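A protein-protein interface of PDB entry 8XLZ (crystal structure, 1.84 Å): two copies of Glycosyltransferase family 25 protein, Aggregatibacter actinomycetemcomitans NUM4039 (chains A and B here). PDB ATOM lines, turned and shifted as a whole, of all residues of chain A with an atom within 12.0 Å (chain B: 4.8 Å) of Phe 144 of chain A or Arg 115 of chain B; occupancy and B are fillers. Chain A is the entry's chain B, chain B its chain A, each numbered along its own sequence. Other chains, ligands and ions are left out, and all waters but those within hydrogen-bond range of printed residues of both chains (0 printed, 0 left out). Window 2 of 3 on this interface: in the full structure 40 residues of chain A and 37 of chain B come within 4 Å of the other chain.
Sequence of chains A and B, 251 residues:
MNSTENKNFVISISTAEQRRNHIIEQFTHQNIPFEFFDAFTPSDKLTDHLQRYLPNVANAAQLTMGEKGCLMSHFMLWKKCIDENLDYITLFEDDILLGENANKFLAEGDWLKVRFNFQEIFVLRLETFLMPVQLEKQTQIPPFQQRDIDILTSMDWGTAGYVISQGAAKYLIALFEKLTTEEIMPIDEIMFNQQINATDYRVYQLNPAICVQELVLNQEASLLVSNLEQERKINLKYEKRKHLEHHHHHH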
ATOM      1  N   LYS A 137      -6.431 -41.237 -24.084  1.00  0.00           N
ATOM      2  CA  LYS A 137      -5.395 -40.371 -23.552  1.00  0.00           C
ATOM      3  C   LYS A 137      -4.160 -40.427 -24.447  1.00  0.00           C
ATOM      4  O   LYS A 137      -3.924 -41.415 -25.142  1.00  0.00           O
ATOM      5  CB  LYS A 137      -5.032 -40.765 -22.118  1.00  0.00           C
ATOM      6  CG  LYS A 137      -6.174 -40.623 -21.129  1.00  0.00           C
ATOM      7  CD  LYS A 137      -6.720 -39.203 -21.136  1.00  0.00           C
ATOM      8  CE  LYS A 137      -7.583 -38.893 -19.941  1.00  0.00           C
ATOM      9  NZ  LYS A 137      -8.185 -37.553 -20.158  1.00  0.00           N
ATOM     10  N   GLN A 138      -3.392 -39.348 -24.455  1.00  0.00           N
ATOM     11  CA  GLN A 138      -2.060 -39.384 -25.066  1.00  0.00           C
ATOM     12  C   GLN A 138      -1.121 -38.566 -24.205  1.00  0.00           C
ATOM     13  O   GLN A 138      -1.551 -37.667 -23.498  1.00  0.00           O
ATOM     14  CB  GLN A 138      -2.061 -38.925 -26.531  1.00  0.00           C
ATOM     15  CG  GLN A 138      -2.546 -37.510 -26.762  1.00  0.00           C
ATOM     16  CD  GLN A 138      -1.557 -36.446 -26.342  1.00  0.00           C
ATOM     17  OE1 GLN A 138      -0.358 -36.528 -26.625  1.00  0.00           O
ATOM     18  NE2 GLN A 138      -2.064 -35.419 -25.686  1.00  0.00           N
ATOM     19  N   THR A 139       0.150 -38.931 -24.275  1.00  0.00           N
ATOM     20  CA  THR A 139       1.169 -38.458 -23.348  1.00  0.00           C
ATOM     21  C   THR A 139       2.201 -37.526 -23.959  1.00  0.00           C
ATOM     22  O   THR A 139       2.965 -36.922 -23.227  1.00  0.00           O
ATOM     23  CB  THR A 139       1.933 -39.655 -22.746  1.00  0.00           C
ATOM     24  OG1 THR A 139       2.376 -40.523 -23.804  1.00  0.00           O
ATOM     25  CG2 THR A 139       1.036 -40.417 -21.790  1.00  0.00           C
ATOM     26  N   GLN A 140       2.218 -37.403 -25.282  1.00  0.00           N
ATOM     27  CA  GLN A 140       3.276 -36.657 -25.965  1.00  0.00           C
ATOM     28  C   GLN A 140       3.020 -35.156 -25.994  1.00  0.00           C
ATOM     29  O   GLN A 140       3.957 -34.370 -25.925  1.00  0.00           O
ATOM     30  CB  GLN A 140       3.451 -37.193 -27.395  1.00  0.00           C
ATOM     31  CG  GLN A 140       4.164 -38.544 -27.464  1.00  0.00           C
ATOM     32  CD  GLN A 140       3.255 -39.772 -27.349  1.00  0.00           C
ATOM     33  OE1 GLN A 140       2.026 -39.673 -27.198  1.00  0.00           O
ATOM     34  NE2 GLN A 140       3.870 -40.952 -27.431  1.00  0.00           N
ATOM     35  N   ILE A 141       1.758 -34.770 -26.155  1.00  0.00           N
ATOM     36  CA  ILE A 141       1.363 -33.369 -26.135  1.00  0.00           C
ATOM     37  C   ILE A 141       0.808 -33.057 -24.749  1.00  0.00           C
ATOM     38  O   ILE A 141      -0.219 -33.612 -24.354  1.00  0.00           O
ATOM     39  CB  ILE A 141       0.316 -33.049 -27.232  1.00  0.00           C
ATOM     40  CG1 ILE A 141       0.927 -33.312 -28.616  1.00  0.00           C
ATOM     41  CG2 ILE A 141      -0.083 -31.580 -27.168  1.00  0.00           C
ATOM     42  CD1 ILE A 141      -0.070 -33.435 -29.748  1.00  0.00           C
ATOM     43  N   PRO A 142       1.464 -32.150 -23.999  1.00  0.00           N
ATOM     44  CA  PRO A 142       0.972 -31.898 -22.643  1.00  0.00           C
ATOM     45  C   PRO A 142      -0.376 -31.192 -22.559  1.00  0.00           C
ATOM     46  O   PRO A 142      -0.732 -30.430 -23.462  1.00  0.00           O
ATOM     47  CB  PRO A 142       2.057 -30.988 -22.029  1.00  0.00           C
ATOM     48  CG  PRO A 142       3.247 -31.110 -22.910  1.00  0.00           C
ATOM     49  CD  PRO A 142       2.697 -31.392 -24.283  1.00  0.00           C
ATOM     50  N   PRO A 143      -1.110 -31.406 -21.449  1.00  0.00           N
ATOM     51  CA  PRO A 143      -2.341 -30.653 -21.208  1.00  0.00           C
ATOM     52  C   PRO A 143      -2.086 -29.169 -21.136  1.00  0.00           C
ATOM     53  O   PRO A 143      -0.943 -28.748 -21.030  1.00  0.00           O
ATOM     54  CB  PRO A 143      -2.822 -31.172 -19.840  1.00  0.00           C
ATOM     55  CG  PRO A 143      -1.589 -31.698 -19.192  1.00  0.00           C
ATOM     56  CD  PRO A 143      -0.802 -32.303 -20.314  1.00  0.00           C
ATOM     57  N   PHE A 144      -3.150 -28.388 -21.214  1.00  0.00           N
ATOM     58  CA  PHE A 144      -3.077 -26.947 -21.056  1.00  0.00           C
ATOM     59  C   PHE A 144      -4.241 -26.453 -20.203  1.00  0.00           C
ATOM     60  O   PHE A 144      -5.408 -26.769 -20.487  1.00  0.00           O
ATOM     61  CB  PHE A 144      -3.110 -26.258 -22.431  1.00  0.00           C
ATOM     62  CG  PHE A 144      -2.925 -24.766 -22.368  1.00  0.00           C
ATOM     63  CD1 PHE A 144      -1.757 -24.236 -21.824  1.00  0.00           C
ATOM     64  CD2 PHE A 144      -3.895 -23.892 -22.842  1.00  0.00           C
ATOM     65  CE1 PHE A 144      -1.560 -22.859 -21.767  1.00  0.00           C
ATOM     66  CE2 PHE A 144      -3.709 -22.513 -22.781  1.00  0.00           C
ATOM     67  CZ  PHE A 144      -2.541 -21.993 -22.238  1.00  0.00           C
ATOM     68  N   GLN A 145      -3.925 -25.683 -19.158  1.00  0.00           N
ATOM     69  CA  GLN A 145      -4.944 -25.136 -18.248  1.00  0.00           C
ATOM     70  C   GLN A 145      -5.851 -26.237 -17.724  1.00  0.00           C
ATOM     71  O   GLN A 145      -7.075 -26.119 -17.761  1.00  0.00           O
ATOM     72  CB  GLN A 145      -5.764 -24.064 -18.959  1.00  0.00           C
ATOM     73  CG  GLN A 145      -4.922 -22.882 -19.388  1.00  0.00           C
ATOM     74  CD  GLN A 145      -4.586 -21.986 -18.222  1.00  0.00           C
ATOM     75  OE1 GLN A 145      -5.461 -21.643 -17.441  1.00  0.00           O
ATOM     76  NE2 GLN A 145      -3.330 -21.574 -18.110  1.00  0.00           N
ATOM     77  N   GLN A 146      -5.226 -27.322 -17.283  1.00  0.00           N
ATOM     78  CA  GLN A 146      -5.917 -28.498 -16.763  1.00  0.00           C
ATOM     79  C   GLN A 146      -6.965 -29.104 -17.713  1.00  0.00           C
ATOM     80  O   GLN A 146      -7.955 -29.693 -17.281  1.00  0.00           O
ATOM     81  CB  GLN A 146      -6.493 -28.186 -15.382  1.00  0.00           C
ATOM     82  CG  GLN A 146      -5.378 -27.982 -14.355  1.00  0.00           C
ATOM     83  CD  GLN A 146      -5.480 -26.667 -13.617  1.00  0.00           C
ATOM     84  OE1 GLN A 146      -5.435 -26.640 -12.381  1.00  0.00           O
ATOM     85  NE2 GLN A 146      -5.607 -25.563 -14.357  1.00  0.00           N
ATOM     86  N   ARG A 147      -6.704 -28.993 -19.011  1.00  0.00           N
ATOM     87  CA  ARG A 147      -7.512 -29.684 -20.002  1.00  0.00           C
ATOM     88  C   ARG A 147      -6.632 -30.578 -20.828  1.00  0.00           C
ATOM     89  O   ARG A 147      -5.584 -30.161 -21.342  1.00  0.00           O
ATOM     90  CB  ARG A 147      -8.273 -28.686 -20.856  1.00  0.00           C
ATOM     91  CG  ARG A 147      -8.948 -27.641 -20.000  1.00  0.00           C
ATOM     92  CD  ARG A 147     -10.297 -27.260 -20.506  1.00  0.00           C
ATOM     93  NE  ARG A 147     -10.746 -26.045 -19.845  1.00  0.00           N
ATOM     94  CZ  ARG A 147     -12.009 -25.664 -19.788  1.00  0.00           C
ATOM     95  NH1 ARG A 147     -12.963 -26.406 -20.345  1.00  0.00           N
ATOM     96  NH2 ARG A 147     -12.323 -24.533 -19.179  1.00  0.00           N
ATOM     97  N   ASP A 148      -7.043 -31.836 -20.904  1.00  0.00           N
ATOM     98  CA  ASP A 148      -6.304 -32.818 -21.646  1.00  0.00           C
ATOM     99  C   ASP A 148      -6.584 -32.652 -23.124  1.00  0.00           C
ATOM    100  O   ASP A 148      -7.630 -32.111 -23.524  1.00  0.00           O
ATOM    101  CB  ASP A 148      -6.673 -34.225 -21.206  1.00  0.00           C
ATOM    102  CG  ASP A 148      -6.032 -34.619 -19.875  1.00  0.00           C
ATOM    103  OD1 ASP A 148      -5.102 -33.948 -19.419  1.00  0.00           O
ATOM    104  OD2 ASP A 148      -6.458 -35.621 -19.292  1.00  0.00           O
ATOM    105  N   ILE A 149      -5.625 -33.110 -23.920  1.00  0.00           N
ATOM    106  CA  ILE A 149      -5.775 -33.163 -25.348  1.00  0.00           C
ATOM    107  C   ILE A 149      -5.847 -34.629 -25.663  1.00  0.00           C
ATOM    108  O   ILE A 149      -4.834 -35.309 -25.692  1.00  0.00           O
ATOM    109  CB  ILE A 149      -4.640 -32.428 -26.084  1.00  0.00           C
ATOM    110  CG1 ILE A 149      -4.763 -30.931 -25.814  1.00  0.00           C
ATOM    111  CG2 ILE A 149      -4.745 -32.658 -27.588  1.00  0.00           C
ATOM    112  CD1 ILE A 149      -3.510 -30.145 -26.080  1.00  0.00           C
ATOM    113  N   ASP A 150      -7.078 -35.117 -25.839  1.00  0.00           N
ATOM    114  CA  ASP A 150      -7.331 -36.529 -26.041  1.00  0.00           C
ATOM    115  C   ASP A 150      -7.525 -36.763 -27.509  1.00  0.00           C
ATOM    116  O   ASP A 150      -7.727 -35.825 -28.267  1.00  0.00           O
ATOM    117  CB  ASP A 150      -8.584 -36.974 -25.293  1.00  0.00           C
ATOM    118  CG  ASP A 150      -8.420 -36.922 -23.764  1.00  0.00           C
ATOM    119  OD1 ASP A 150      -7.266 -36.810 -23.270  1.00  0.00           O
ATOM    120  OD2 ASP A 150      -9.447 -36.992 -23.070  1.00  0.00           O
ATOM    121  N   ILE A 151      -7.431 -38.021 -27.901  1.00  0.00           N
ATOM    122  CA  ILE A 151      -7.632 -38.420 -29.276  1.00  0.00           C
ATOM    123  C   ILE A 151      -9.022 -39.057 -29.381  1.00  0.00           C
ATOM    124  O   ILE A 151      -9.351 -39.977 -28.626  1.00  0.00           O
ATOM    125  CB  ILE A 151      -6.556 -39.413 -29.740  1.00  0.00           C
ATOM    126  CG1 ILE A 151      -5.173 -38.779 -29.610  1.00  0.00           C
ATOM    127  CG2 ILE A 151      -6.789 -39.836 -31.194  1.00  0.00           C
ATOM    128  CD1 ILE A 151      -4.045 -39.767 -29.695  1.00  0.00           C
ATOM    129  N   LYS B 104      -8.532 -17.918 -22.602  1.00  0.00           N
ATOM    130  CA  LYS B 104      -7.164 -18.437 -22.425  1.00  0.00           C
ATOM    131  C   LYS B 104      -6.782 -19.293 -23.648  1.00  0.00           C
ATOM    132  O   LYS B 104      -5.604 -19.466 -23.974  1.00  0.00           O
ATOM    133  CB  LYS B 104      -7.011 -19.323 -21.165  1.00  0.00           C
ATOM    134  CG  LYS B 104      -7.659 -18.873 -19.859  1.00  0.00           C
ATOM    135  CD  LYS B 104      -7.117 -17.558 -19.347  1.00  0.00           C
ATOM    136  CE  LYS B 104      -7.172 -17.512 -17.821  1.00  0.00           C
ATOM    137  NZ  LYS B 104      -6.951 -16.128 -17.323  1.00  0.00           N
ATOM    138  N   PHE B 105      -7.800 -19.848 -24.304  1.00  0.00           N
ATOM    139  CA  PHE B 105      -7.610 -20.743 -25.428  1.00  0.00           C
ATOM    140  C   PHE B 105      -7.749 -20.033 -26.782  1.00  0.00           C
ATOM    141  O   PHE B 105      -7.089 -20.412 -27.729  1.00  0.00           O
ATOM    142  CB  PHE B 105      -8.608 -21.892 -25.342  1.00  0.00           C
ATOM    143  CG  PHE B 105      -8.502 -22.695 -24.085  1.00  0.00           C
ATOM    144  CD1 PHE B 105      -9.161 -22.297 -22.934  1.00  0.00           C
ATOM    145  CD2 PHE B 105      -7.725 -23.828 -24.041  1.00  0.00           C
ATOM    146  CE1 PHE B 105      -9.066 -23.036 -21.776  1.00  0.00           C
ATOM    147  CE2 PHE B 105      -7.616 -24.567 -22.881  1.00  0.00           C
ATOM    148  CZ  PHE B 105      -8.283 -24.167 -21.740  1.00  0.00           C
ATOM    149  N   TRP B 111      -0.184 -21.278 -26.894  1.00  0.00           N
ATOM    150  CA  TRP B 111      -0.373 -22.634 -26.369  1.00  0.00           C
ATOM    151  C   TRP B 111      -0.466 -23.683 -27.489  1.00  0.00           C
ATOM    152  O   TRP B 111       0.012 -24.793 -27.340  1.00  0.00           O
ATOM    153  CB  TRP B 111      -1.578 -22.690 -25.444  1.00  0.00           C
ATOM    154  CG  TRP B 111      -2.901 -22.654 -26.129  1.00  0.00           C
ATOM    155  CD1 TRP B 111      -3.551 -21.551 -26.597  1.00  0.00           C
ATOM    156  CD2 TRP B 111      -3.750 -23.762 -26.380  1.00  0.00           C
ATOM    157  NE1 TRP B 111      -4.748 -21.916 -27.154  1.00  0.00           N
ATOM    158  CE2 TRP B 111      -4.905 -23.267 -27.019  1.00  0.00           C
ATOM    159  CE3 TRP B 111      -3.645 -25.137 -26.142  1.00  0.00           C
ATOM    160  CZ2 TRP B 111      -5.950 -24.092 -27.417  1.00  0.00           C
ATOM    161  CZ3 TRP B 111      -4.684 -25.960 -26.544  1.00  0.00           C
ATOM    162  CH2 TRP B 111      -5.827 -25.433 -27.157  1.00  0.00           C
ATOM    163  N   LEU B 112      -1.034 -23.311 -28.627  1.00  0.00           N
ATOM    164  CA  LEU B 112      -1.015 -24.199 -29.813  1.00  0.00           C
ATOM    165  C   LEU B 112       0.342 -24.267 -30.503  1.00  0.00           C
ATOM    166  O   LEU B 112       0.799 -25.341 -30.911  1.00  0.00           O
ATOM    167  CB  LEU B 112      -2.045 -23.721 -30.839  1.00  0.00           C
ATOM    168  CG  LEU B 112      -3.478 -23.622 -30.349  1.00  0.00           C
ATOM    169  CD1 LEU B 112      -4.316 -22.686 -31.212  1.00  0.00           C
ATOM    170  CD2 LEU B 112      -4.078 -25.008 -30.311  1.00  0.00           C
ATOM    171  N   LYS B 113       0.957 -23.119 -30.672  1.00  0.00           N
ATOM    172  CA  LYS B 113       2.251 -23.026 -31.396  1.00  0.00           C
ATOM    173  C   LYS B 113       3.372 -23.757 -30.678  1.00  0.00           C
ATOM    174  O   LYS B 113       4.266 -24.291 -31.314  1.00  0.00           O
ATOM    175  CB  LYS B 113       2.682 -21.585 -31.599  1.00  0.00           C
ATOM    176  CG  LYS B 113       1.705 -20.741 -32.397  1.00  0.00           C
ATOM    177  CD  LYS B 113       2.240 -19.337 -32.645  1.00  0.00           C
ATOM    178  CE  LYS B 113       1.159 -18.257 -32.586  1.00  0.00           C
ATOM    179  NZ  LYS B 113      -0.063 -18.587 -33.382  1.00  0.00           N
ATOM    180  N   VAL B 114       3.322 -23.811 -29.353  1.00  0.00           N
ATOM    181  CA  VAL B 114       4.331 -24.606 -28.637  1.00  0.00           C
ATOM    182  C   VAL B 114       3.988 -26.096 -28.561  1.00  0.00           C
ATOM    183  O   VAL B 114       4.824 -26.895 -28.146  1.00  0.00           O
ATOM    184  CB  VAL B 114       4.651 -24.034 -27.244  1.00  0.00           C
ATOM    185  CG1 VAL B 114       4.976 -22.542 -27.361  1.00  0.00           C
ATOM    186  CG2 VAL B 114       3.514 -24.274 -26.251  1.00  0.00           C
ATOM    187  N   ARG B 115       2.774 -26.475 -28.968  1.00  0.00           N
ATOM    188  CA  ARG B 115       2.343 -27.875 -28.876  1.00  0.00           C
ATOM    189  C   ARG B 115       2.365 -28.651 -30.168  1.00  0.00           C
ATOM    190  O   ARG B 115       2.741 -29.836 -30.179  1.00  0.00           O
ATOM    191  CB  ARG B 115       0.934 -27.977 -28.281  1.00  0.00           C
ATOM    192  CG  ARG B 115       0.960 -27.989 -26.764  1.00  0.00           C
ATOM    193  CD  ARG B 115      -0.388 -27.802 -26.104  1.00  0.00           C
ATOM    194  NE  ARG B 115      -0.148 -27.796 -24.664  1.00  0.00           N
ATOM    195  CZ  ARG B 115       0.308 -26.754 -23.967  1.00  0.00           C
ATOM    196  NH1 ARG B 115       0.542 -25.586 -24.553  1.00  0.00           N
ATOM    197  NH2 ARG B 115       0.531 -26.908 -22.657  1.00  0.00           N
ATOM    198  N   PHE B 116       1.944 -28.010 -31.254  1.00  0.00           N
ATOM    199  CA  PHE B 116       1.756 -28.721 -32.518  1.00  0.00           C
ATOM    200  C   PHE B 116       2.651 -28.247 -33.628  1.00  0.00           C
ATOM    201  O   PHE B 116       3.009 -27.087 -33.693  1.00  0.00           O
ATOM    202  CB  PHE B 116       0.329 -28.544 -32.996  1.00  0.00           C
ATOM    203  CG  PHE B 116      -0.714 -28.998 -32.026  1.00  0.00           C
ATOM    204  CD1 PHE B 116      -1.120 -30.334 -31.960  1.00  0.00           C
ATOM    205  CD2 PHE B 116      -1.311 -28.087 -31.183  1.00  0.00           C
ATOM    206  CE1 PHE B 116      -2.109 -30.727 -31.065  1.00  0.00           C
ATOM    207  CE2 PHE B 116      -2.293 -28.479 -30.290  1.00  0.00           C
ATOM    208  CZ  PHE B 116      -2.688 -29.801 -30.235  1.00  0.00           C
ATOM    209  N   ASN B 117       2.990 -29.173 -34.504  1.00  0.00           N
ATOM    210  CA  ASN B 117       3.526 -28.870 -35.827  1.00  0.00           C
ATOM    211  C   ASN B 117       2.339 -28.741 -36.798  1.00  0.00           C
ATOM    212  O   ASN B 117       1.706 -29.737 -37.074  1.00  0.00           O
ATOM    213  CB  ASN B 117       4.422 -30.043 -36.234  1.00  0.00           C
ATOM    214  CG  ASN B 117       4.957 -29.940 -37.655  1.00  0.00           C
ATOM    215  OD1 ASN B 117       4.677 -28.984 -38.400  1.00  0.00           O
ATOM    216  ND2 ASN B 117       5.696 -30.952 -38.051  1.00  0.00           N
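Among the printed residues, pairs that only touch across the chains: Ile 141 of chain A with Arg 115 of chain B (3.8 Å), Ile 141 of chain A with Phe 116 of chain B (3.6 Å), Phe 144 of chain A with Lys 104 of chain B (3.8 Å), Phe 144 of chain A with Phe 105 of chain B (3.8 Å), Phe 144 of chain A with Trp 111 of chain B (3.4 Å), Phe 144 of chain A with Arg 115 of chain B (3.6 Å), Gln 145 of chain A with Phe 105 of chain B (3.8 Å), Arg 147 of chain A with Phe 105 of chain B (3.6 Å) and Ile 149 of chain A with Arg 115 of chain B (3.9 Å).
No position is printed for both chains.
Of the 11 pairs that touch across the chains among the printed residues, none has its exchanged pair printed and touching as well.
O of Phe 105 of chain B lies within hydrogen-bond range of NE1 of Trp 111 of chain B (2.8 Å).
The backbone NH of Ile 141 of chain A lies within hydrogen-bond range of the side-chain amide oxygen of Gln 138 of chain A (2.8 Å).
The backbone carbonyl oxygen (O) of Trp 111 of chain B is in hydrogen-bond range of the guanidinium group (NH1) of Arg 115 of chain B (2.9 Å).
The side-chain amide nitrogen (NE2) of Gln 138 of chain A is in hydrogen-bond range of the backbone carbonyl oxygen (O) of Ile 149 of chain A, at 2.8 Å.
O of Pro 143 of chain A lies within hydrogen-bond range of NH2 of Arg 115 of chain B (2.9 Å).
The backbone carbonyl oxygen (O) of Pro 142 of chain A lies within hydrogen-bond range of the guanidinium group (NE) of Arg 115 of chain B (3.0 Å).
Of the 9 printed residues of chain B, 5 touch a printed residue of chain A.
Of the 15 printed residues of chain A, 7 touch a printed residue of chain B.
Printed residues of chain A that touch a printed residue of chain B: Ile 141, Pro 142, Pro 143, Phe 144, Gln 145, Arg 147 and Ile 149.
Hydrophobic or aromatic side chains of chain A within 4 Å of the printed part of chain B: Ile 141, Phe 144 and Ile 149.
Among the printed residues, no Asp or Glu carboxylate lies within 4 Å of a Lys or Arg side-chain nitrogen of the other chain.
Of chain B, only Lys 104, Phe 105, Trp 111 and Arg 115 come within 4 Å of Phe 144 of chain A.
Arg 115 of chain B touches just these residues of chain A: Ile 141 (3.8 Å), Pro 142 (3.0 Å), Pro 143 (2.9 Å), Phe 144 (3.6 Å) and Ile 149 (3.9 Å).
Phe 105 of chain B touches just these residues of chain A: Phe 144 (3.8 Å), Gln 145 (3.8 Å) and Arg 147 (3.6 Å).
Trp 111 of chain B touches one residue of chain A.
No residue of chain A comes within 4 Å of Val 114 of chain B.
Of chain A, only Ile 141 comes within 4 Å of Phe 116 of chain B.
Printed residues of chain A within 4 Å of Lys 104 of chain B: Phe 144.
Of the printed residues of chain B, Gln 145 of chain A touches Phe 105.
The nearest printed residue of chain B that does not touch Phe 144 of chain A is Leu 112 of chain B (6.5 Å).
The nearest residue of chain A that does not touch Arg 115 of chain B is Gln 145 of chain A (5.8 Å).
The nearest printed residue of chain A that does not touch Lys 104 of chain B is Gln 145 of chain A (4.3 Å).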
